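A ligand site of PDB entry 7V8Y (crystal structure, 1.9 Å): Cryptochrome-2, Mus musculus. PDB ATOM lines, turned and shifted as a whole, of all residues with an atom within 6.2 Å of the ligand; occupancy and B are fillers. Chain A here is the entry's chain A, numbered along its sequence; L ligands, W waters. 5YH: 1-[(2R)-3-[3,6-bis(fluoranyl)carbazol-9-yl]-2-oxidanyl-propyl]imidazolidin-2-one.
Trp 312 touches the ligand (CE3 to C06, 3.4 Å).
CE2 of Phe 316 touches O01 of the ligand, at 3.8 Å.
CG of His 375 touches C10 of the ligand, at 3.5 Å.
NH1 of Arg 378 touches C21 of the ligand, at 3.0 Å.
Ala 382 touches the ligand.
Phe 401 touches the ligand (CE2 to C17, 3.96 Å).
CD1 of Leu 405 touches F25 of the ligand, at 3.8 Å.
Asp 407 touches the ligand (OD1 to C22, 3.9 Å).
Ala 408 touches the ligand.
Val 412 touches the ligand.
CA of Asn 413 touches F25 of the ligand, 3.2 Å away.
CD2 of Trp 417 touches F16 of the ligand, at 3.6 Å.
Trp 419 touches the ligand.
Leu 420 touches the ligand (CB to F16, 3.6 Å).
16 residues have an atom within 4 Å of the ligand: Trp 312, Phe 316, His 375, Arg 378, His 379, Ala 382, Phe 401, Leu 405, Asp 407, Ala 408, Val 412, Asn 413, Ser 416, Trp 417, Trp 419 and Leu 420.
The nearest printed residue that does not touch the ligand is Asp 409 (4.3 Å).
An oxygen (O01) of the ligand sits at hydrogen-bond distance from the side-chain hydroxyl of Ser 416.
NE2 of His 379 lies within hydrogen-bond range of O09 of the ligand, 3.1 Å away.
The side-chain carboxylate (OD1) of Asp 409 sits at hydrogen-bond distance from the backbone NH (N) of Val 412, 2.9 Å away.
NE1 of Trp 417 sits close to OD1 of Asn 413, 3.0 Å away.
OD1 of Asp 407 lies within salt-bridge range of NH1 of Arg 378 (2.8 Å).
The backbone carbonyl oxygen of Val 412 lies within hydrogen-bond range of the side-chain hydroxyl of Ser 416 (2.6 Å).
O of Trp 417 lies within hydrogen-bond range of OG of Ser 421.
ND1 of His 379 lies within hydrogen-bond range of O of His 375, at 2.9 Å.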
ATOM      1  N   TRP A 312      30.581  23.939  -5.568  1.00  0.00           N
ATOM      2  CA  TRP A 312      29.901  22.920  -4.780  1.00  0.00           C
ATOM      3  C   TRP A 312      29.809  21.613  -5.549  1.00  0.00           C
ATOM      4  O   TRP A 312      29.996  20.527  -4.992  1.00  0.00           O
ATOM      5  CB  TRP A 312      28.490  23.405  -4.352  1.00  0.00           C
ATOM      6  CG  TRP A 312      28.580  24.196  -3.058  1.00  0.00           C
ATOM      7  CD1 TRP A 312      28.624  25.563  -2.922  1.00  0.00           C
ATOM      8  CD2 TRP A 312      28.691  23.653  -1.728  1.00  0.00           C
ATOM      9  NE1 TRP A 312      28.750  25.904  -1.582  1.00  0.00           N
ATOM     10  CE2 TRP A 312      28.785  24.752  -0.827  1.00  0.00           C
ATOM     11  CE3 TRP A 312      28.721  22.343  -1.219  1.00  0.00           C
ATOM     12  CZ2 TRP A 312      28.914  24.581   0.552  1.00  0.00           C
ATOM     13  CZ3 TRP A 312      28.842  22.174   0.163  1.00  0.00           C
ATOM     14  CH2 TRP A 312      28.944  23.291   1.032  1.00  0.00           C
ATOM     15  N   PHE A 316      31.540  17.964  -4.313  1.00  0.00           N
ATOM     16  CA  PHE A 316      30.949  16.630  -4.183  1.00  0.00           C
ATOM     17  C   PHE A 316      31.647  15.625  -5.091  1.00  0.00           C
ATOM     18  O   PHE A 316      31.780  14.449  -4.722  1.00  0.00           O
ATOM     19  CB  PHE A 316      29.469  16.700  -4.496  1.00  0.00           C
ATOM     20  CG  PHE A 316      28.669  17.403  -3.418  1.00  0.00           C
ATOM     21  CD1 PHE A 316      28.832  17.043  -2.058  1.00  0.00           C
ATOM     22  CD2 PHE A 316      27.810  18.444  -3.726  1.00  0.00           C
ATOM     23  CE1 PHE A 316      28.123  17.677  -1.047  1.00  0.00           C
ATOM     24  CE2 PHE A 316      27.090  19.102  -2.700  1.00  0.00           C
ATOM     25  CZ  PHE A 316      27.274  18.715  -1.357  1.00  0.00           C
ATOM     26  N   HIS A 375      16.936  24.473  -5.873  1.00  0.00           N
ATOM     27  CA  HIS A 375      17.755  23.921  -4.795  1.00  0.00           C
ATOM     28  C   HIS A 375      17.097  24.072  -3.424  1.00  0.00           C
ATOM     29  O   HIS A 375      17.206  23.181  -2.568  1.00  0.00           O
ATOM     30  CB  HIS A 375      19.132  24.601  -4.771  1.00  0.00           C
ATOM     31  CG  HIS A 375      20.061  24.089  -5.827  1.00  0.00           C
ATOM     32  ND1 HIS A 375      21.369  24.516  -5.937  1.00  0.00           N
ATOM     33  CD2 HIS A 375      19.873  23.174  -6.807  1.00  0.00           C
ATOM     34  CE1 HIS A 375      21.944  23.913  -6.965  1.00  0.00           C
ATOM     35  NE2 HIS A 375      21.066  23.076  -7.498  1.00  0.00           N
ATOM     36  N   LEU A 376      16.412  25.182  -3.182  1.00  0.00           N
ATOM     37  CA  LEU A 376      15.783  25.334  -1.870  1.00  0.00           C
ATOM     38  C   LEU A 376      14.566  24.409  -1.730  1.00  0.00           C
ATOM     39  O   LEU A 376      14.240  23.986  -0.608  1.00  0.00           O
ATOM     40  CB  LEU A 376      15.414  26.786  -1.641  1.00  0.00           C
ATOM     41  CG  LEU A 376      16.639  27.691  -1.474  1.00  0.00           C
ATOM     42  CD1 LEU A 376      16.192  29.105  -1.126  1.00  0.00           C
ATOM     43  CD2 LEU A 376      17.646  27.134  -0.451  1.00  0.00           C
ATOM     44  N   ARG A 378      14.656  21.390  -3.020  1.00  0.00           N
ATOM     45  CA  ARG A 378      15.309  20.129  -2.666  1.00  0.00           C
ATOM     46  C   ARG A 378      15.607  20.064  -1.176  1.00  0.00           C
ATOM     47  O   ARG A 378      15.405  19.014  -0.544  1.00  0.00           O
ATOM     48  CB  ARG A 378      16.604  19.968  -3.468  1.00  0.00           C
ATOM     49  CG  ARG A 378      16.366  19.973  -4.946  1.00  0.00           C
ATOM     50  CD  ARG A 378      17.696  19.947  -5.778  1.00  0.00           C
ATOM     51  NE  ARG A 378      17.442  20.512  -7.104  1.00  0.00           N
ATOM     52  CZ  ARG A 378      18.200  20.313  -8.193  1.00  0.00           C
ATOM     53  NH1 ARG A 378      19.330  19.605  -8.104  1.00  0.00           N
ATOM     54  NH2 ARG A 378      17.837  20.871  -9.349  1.00  0.00           N
ATOM     55  N   HIS A 379      16.112  21.160  -0.600  1.00  0.00           N
ATOM     56  CA  HIS A 379      16.267  21.223   0.850  1.00  0.00           C
ATOM     57  C   HIS A 379      14.935  20.871   1.536  1.00  0.00           C
ATOM     58  O   HIS A 379      14.882  20.039   2.445  1.00  0.00           O
ATOM     59  CB  HIS A 379      16.716  22.617   1.313  1.00  0.00           C
ATOM     60  CG  HIS A 379      18.100  23.028   0.886  1.00  0.00           C
ATOM     61  ND1 HIS A 379      18.760  22.514  -0.209  1.00  0.00           N
ATOM     62  CD2 HIS A 379      18.932  23.973   1.406  1.00  0.00           C
ATOM     63  CE1 HIS A 379      19.927  23.109  -0.357  1.00  0.00           C
ATOM     64  NE2 HIS A 379      20.063  23.997   0.623  1.00  0.00           N
ATOM     65  N   ALA A 382      13.923  17.086   1.017  1.00  0.00           N
ATOM     66  CA  ALA A 382      14.879  16.154   1.617  1.00  0.00           C
ATOM     67  C   ALA A 382      14.820  16.230   3.140  1.00  0.00           C
ATOM     68  O   ALA A 382      14.970  15.198   3.823  1.00  0.00           O
ATOM     69  CB  ALA A 382      16.299  16.481   1.135  1.00  0.00           C
ATOM     70  N   CYS A 383      14.637  17.440   3.670  1.00  0.00           N
ATOM     71  CA  CYS A 383      14.414  17.627   5.094  1.00  0.00           C
ATOM     72  C   CYS A 383      13.194  16.853   5.542  1.00  0.00           C
ATOM     73  O   CYS A 383      13.222  16.133   6.552  1.00  0.00           O
ATOM     74  CB  CYS A 383      14.203  19.116   5.391  1.00  0.00           C
ATOM     75  SG  CYS A 383      15.765  19.889   5.726  1.00  0.00           S
ATOM     76  N   PHE A 401      15.496  10.764  -6.411  1.00  0.00           N
ATOM     77  CA  PHE A 401      16.072  11.824  -7.234  1.00  0.00           C
ATOM     78  C   PHE A 401      16.826  11.248  -8.438  1.00  0.00           C
ATOM     79  O   PHE A 401      16.837  11.871  -9.514  1.00  0.00           O
ATOM     80  CB  PHE A 401      17.033  12.670  -6.391  1.00  0.00           C
ATOM     81  CG  PHE A 401      16.364  13.801  -5.606  1.00  0.00           C
ATOM     82  CD1 PHE A 401      15.012  13.744  -5.267  1.00  0.00           C
ATOM     83  CD2 PHE A 401      17.114  14.925  -5.241  1.00  0.00           C
ATOM     84  CE1 PHE A 401      14.393  14.807  -4.539  1.00  0.00           C
ATOM     85  CE2 PHE A 401      16.514  15.982  -4.518  1.00  0.00           C
ATOM     86  CZ  PHE A 401      15.153  15.928  -4.177  1.00  0.00           C
ATOM     87  N   LEU A 405      15.318  13.423 -11.240  1.00  0.00           N
ATOM     88  CA  LEU A 405      16.015  14.715 -11.325  1.00  0.00           C
ATOM     89  C   LEU A 405      16.985  14.754 -12.501  1.00  0.00           C
ATOM     90  O   LEU A 405      17.959  13.987 -12.533  1.00  0.00           O
ATOM     91  CB  LEU A 405      16.816  15.008 -10.066  1.00  0.00           C
ATOM     92  CG  LEU A 405      16.535  16.117  -9.086  1.00  0.00           C
ATOM     93  CD1 LEU A 405      17.795  16.338  -8.301  1.00  0.00           C
ATOM     94  CD2 LEU A 405      16.015  17.386  -9.729  1.00  0.00           C
ATOM     95  N   ASP A 407      19.418  16.758 -13.089  1.00  0.00           N
ATOM     96  CA  ASP A 407      20.798  17.115 -12.839  1.00  0.00           C
ATOM     97  C   ASP A 407      21.428  16.276 -11.733  1.00  0.00           C
ATOM     98  O   ASP A 407      22.475  16.643 -11.198  1.00  0.00           O
ATOM     99  CB  ASP A 407      20.918  18.617 -12.569  1.00  0.00           C
ATOM    100  CG  ASP A 407      20.133  19.088 -11.323  1.00  0.00           C
ATOM    101  OD1 ASP A 407      19.760  18.248 -10.473  1.00  0.00           O
ATOM    102  OD2 ASP A 407      19.933  20.310 -11.210  1.00  0.00           O
ATOM    103  N   ALA A 408      20.844  15.108 -11.440  1.00  0.00           N
ATOM    104  CA  ALA A 408      21.371  14.196 -10.438  1.00  0.00           C
ATOM    105  C   ALA A 408      22.421  13.285 -11.053  1.00  0.00           C
ATOM    106  O   ALA A 408      22.247  12.763 -12.156  1.00  0.00           O
ATOM    107  CB  ALA A 408      20.283  13.299  -9.833  1.00  0.00           C
ATOM    108  N   ASP A 409      23.518  13.095 -10.327  1.00  0.00           N
ATOM    109  CA  ASP A 409      24.433  12.020 -10.642  1.00  0.00           C
ATOM    110  C   ASP A 409      24.968  11.474  -9.331  1.00  0.00           C
ATOM    111  O   ASP A 409      24.712  12.023  -8.257  1.00  0.00           O
ATOM    112  CB  ASP A 409      25.545  12.488 -11.608  1.00  0.00           C
ATOM    113  CG  ASP A 409      26.367  13.644 -11.084  1.00  0.00           C
ATOM    114  OD1 ASP A 409      26.660  13.683  -9.864  1.00  0.00           O
ATOM    115  OD2 ASP A 409      26.785  14.523 -11.891  1.00  0.00           O
ATOM    116  N   VAL A 412      26.892  14.363  -7.004  1.00  0.00           N
ATOM    117  CA  VAL A 412      26.215  15.505  -6.391  1.00  0.00           C
ATOM    118  C   VAL A 412      24.935  15.075  -5.660  1.00  0.00           C
ATOM    119  O   VAL A 412      24.522  15.733  -4.697  1.00  0.00           O
ATOM    120  CB  VAL A 412      25.916  16.577  -7.448  1.00  0.00           C
ATOM    121  CG1 VAL A 412      27.196  17.102  -8.080  1.00  0.00           C
ATOM    122  CG2 VAL A 412      24.949  16.013  -8.530  1.00  0.00           C
ATOM    123  N   ASN A 413      24.310  13.986  -6.084  1.00  0.00           N
ATOM    124  CA  ASN A 413      23.043  13.561  -5.479  1.00  0.00           C
ATOM    125  C   ASN A 413      23.267  12.985  -4.085  1.00  0.00           C
ATOM    126  O   ASN A 413      22.796  13.525  -3.085  1.00  0.00           O
ATOM    127  CB  ASN A 413      22.351  12.539  -6.408  1.00  0.00           C
ATOM    128  CG  ASN A 413      20.924  12.193  -5.976  1.00  0.00           C
ATOM    129  OD1 ASN A 413      20.317  12.877  -5.130  1.00  0.00           O
ATOM    130  ND2 ASN A 413      20.381  11.139  -6.582  1.00  0.00           N
ATOM    131  N   ALA A 414      24.051  11.912  -3.988  1.00  0.00           N
ATOM    132  CA  ALA A 414      24.375  11.377  -2.677  1.00  0.00           C
ATOM    133  C   ALA A 414      25.102  12.399  -1.819  1.00  0.00           C
ATOM    134  O   ALA A 414      24.830  12.504  -0.615  1.00  0.00           O
ATOM    135  CB  ALA A 414      25.205  10.100  -2.789  1.00  0.00           C
ATOM    136  N   SER A 416      24.887  15.684  -1.750  1.00  0.00           N
ATOM    137  CA  SER A 416      23.948  16.664  -1.249  1.00  0.00           C
ATOM    138  C   SER A 416      23.028  16.076  -0.191  1.00  0.00           C
ATOM    139  O   SER A 416      22.699  16.750   0.783  1.00  0.00           O
ATOM    140  CB  SER A 416      23.117  17.207  -2.408  1.00  0.00           C
ATOM    141  OG  SER A 416      23.929  17.913  -3.319  1.00  0.00           O
ATOM    142  N   TRP A 417      22.576  14.842  -0.397  1.00  0.00           N
ATOM    143  CA  TRP A 417      21.666  14.229   0.564  1.00  0.00           C
ATOM    144  C   TRP A 417      22.357  13.970   1.887  1.00  0.00           C
ATOM    145  O   TRP A 417      21.756  14.143   2.947  1.00  0.00           O
ATOM    146  CB  TRP A 417      21.107  12.941   0.009  1.00  0.00           C
ATOM    147  CG  TRP A 417      19.924  13.123  -0.872  1.00  0.00           C
ATOM    148  CD1 TRP A 417      19.913  13.259  -2.251  1.00  0.00           C
ATOM    149  CD2 TRP A 417      18.565  13.154  -0.454  1.00  0.00           C
ATOM    150  NE1 TRP A 417      18.611  13.389  -2.695  1.00  0.00           N
ATOM    151  CE2 TRP A 417      17.772  13.330  -1.614  1.00  0.00           C
ATOM    152  CE3 TRP A 417      17.932  13.056   0.803  1.00  0.00           C
ATOM    153  CZ2 TRP A 417      16.373  13.421  -1.553  1.00  0.00           C
ATOM    154  CZ3 TRP A 417      16.551  13.141   0.858  1.00  0.00           C
ATOM    155  CH2 TRP A 417      15.786  13.319  -0.319  1.00  0.00           C
ATOM    156  N   MET A 418      23.597  13.489   1.840  1.00  0.00           N
ATOM    157  CA  MET A 418      24.376  13.307   3.075  1.00  0.00           C
ATOM    158  C   MET A 418      24.580  14.642   3.789  1.00  0.00           C
ATOM    159  O   MET A 418      24.431  14.721   5.003  1.00  0.00           O
ATOM    160  CB  MET A 418      25.731  12.642   2.773  1.00  0.00           C
ATOM    161  CG  MET A 418      25.585  11.177   2.398  1.00  0.00           C
ATOM    162  SD  MET A 418      27.132  10.279   2.407  1.00  0.00           S
ATOM    163  CE  MET A 418      27.935  10.992   0.952  1.00  0.00           C
ATOM    164  N   TRP A 419      24.961  15.679   3.031  1.00  0.00           N
ATOM    165  CA  TRP A 419      25.118  17.006   3.612  1.00  0.00           C
ATOM    166  C   TRP A 419      23.830  17.498   4.257  1.00  0.00           C
ATOM    167  O   TRP A 419      23.817  17.963   5.412  1.00  0.00           O
ATOM    168  CB  TRP A 419      25.581  18.004   2.544  1.00  0.00           C
ATOM    169  CG  TRP A 419      25.414  19.439   2.992  1.00  0.00           C
ATOM    170  CD1 TRP A 419      26.216  20.125   3.873  1.00  0.00           C
ATOM    171  CD2 TRP A 419      24.376  20.367   2.585  1.00  0.00           C
ATOM    172  NE1 TRP A 419      25.732  21.413   4.058  1.00  0.00           N
ATOM    173  CE2 TRP A 419      24.617  21.586   3.284  1.00  0.00           C
ATOM    174  CE3 TRP A 419      23.277  20.274   1.729  1.00  0.00           C
ATOM    175  CZ2 TRP A 419      23.791  22.713   3.128  1.00  0.00           C
ATOM    176  CZ3 TRP A 419      22.461  21.398   1.571  1.00  0.00           C
ATOM    177  CH2 TRP A 419      22.722  22.601   2.283  1.00  0.00           C
ATOM    178  N   LEU A 420      22.721  17.430   3.498  1.00  0.00           N
ATOM    179  CA  LEU A 420      21.467  17.993   3.985  1.00  0.00           C
ATOM    180  C   LEU A 420      20.985  17.264   5.239  1.00  0.00           C
ATOM    181  O   LEU A 420      20.474  17.899   6.182  1.00  0.00           O
ATOM    182  CB  LEU A 420      20.420  17.892   2.879  1.00  0.00           C
ATOM    183  CG  LEU A 420      19.001  18.471   3.077  1.00  0.00           C
ATOM    184  CD1 LEU A 420      18.151  17.579   3.976  1.00  0.00           C
ATOM    185  CD2 LEU A 420      19.045  19.885   3.618  1.00  0.00           C
ATOM    186  N   SER A 421      21.119  15.938   5.248  1.00  0.00           N
ATOM    187  CA  SER A 421      20.599  15.124   6.331  1.00  0.00           C
ATOM    188  C   SER A 421      21.526  15.064   7.538  1.00  0.00           C
ATOM    189  O   SER A 421      21.225  14.319   8.470  1.00  0.00           O
ATOM    190  CB  SER A 421      20.303  13.715   5.809  1.00  0.00           C
ATOM    191  OG  SER A 421      21.500  13.013   5.481  1.00  0.00           O
HETATM  192  C10 5YH L   1      21.418  21.226  -4.257  1.00  0.00           C
HETATM  193  C13 5YH L   1      20.053  19.764  -1.789  1.00  0.00           C
HETATM  194  C15 5YH L   1      19.293  17.577  -1.136  1.00  0.00           C
HETATM  195  C17 5YH L   1      19.665  16.981  -2.332  1.00  0.00           C
HETATM  196  C20 5YH L   1      21.229  18.839  -5.164  1.00  0.00           C
HETATM  197  C21 5YH L   1      21.797  18.946  -6.476  1.00  0.00           C
HETATM  198  C22 5YH L   1      21.856  17.801  -7.272  1.00  0.00           C
HETATM  199  C24 5YH L   1      20.775  16.434  -5.493  1.00  0.00           C
HETATM  200  C02 5YH L   1      22.752  21.426  -3.368  1.00  0.00           C
HETATM  201  C03 5YH L   1      23.232  22.900  -3.339  1.00  0.00           C
HETATM  202  C05 5YH L   1      25.177  22.650  -1.716  1.00  0.00           C
HETATM  203  C06 5YH L   1      25.523  23.291  -0.338  1.00  0.00           C
HETATM  204  C08 5YH L   1      23.486  24.142  -1.108  1.00  0.00           C
HETATM  205  C12 5YH L   1      20.432  19.207  -3.046  1.00  0.00           C
HETATM  206  C14 5YH L   1      19.470  18.927  -0.796  1.00  0.00           C
HETATM  207  C18 5YH L   1      20.224  17.815  -3.330  1.00  0.00           C
HETATM  208  C19 5YH L   1      20.723  17.587  -4.678  1.00  0.00           C
HETATM  209  C23 5YH L   1      21.339  16.605  -6.728  1.00  0.00           C
HETATM  210  F16 5YH L   1      18.799  16.733  -0.164  1.00  0.00           F
HETATM  211  F25 5YH L   1      21.386  15.465  -7.490  1.00  0.00           F
HETATM  212  N04 5YH L   1      23.903  23.222  -2.119  1.00  0.00           N
HETATM  213  N07 5YH L   1      24.441  24.198  -0.055  1.00  0.00           N
HETATM  214  N11 5YH L   1      21.030  19.809  -4.160  1.00  0.00           N
HETATM  215  O01 5YH L   1      23.847  20.659  -3.933  1.00  0.00           O
HETATM  216  O09 5YH L   1      22.444  24.803  -1.129  1.00  0.00           O
HETATM  217  O   HOH W   1      25.353  20.741  -6.387  1.00  0.00           O
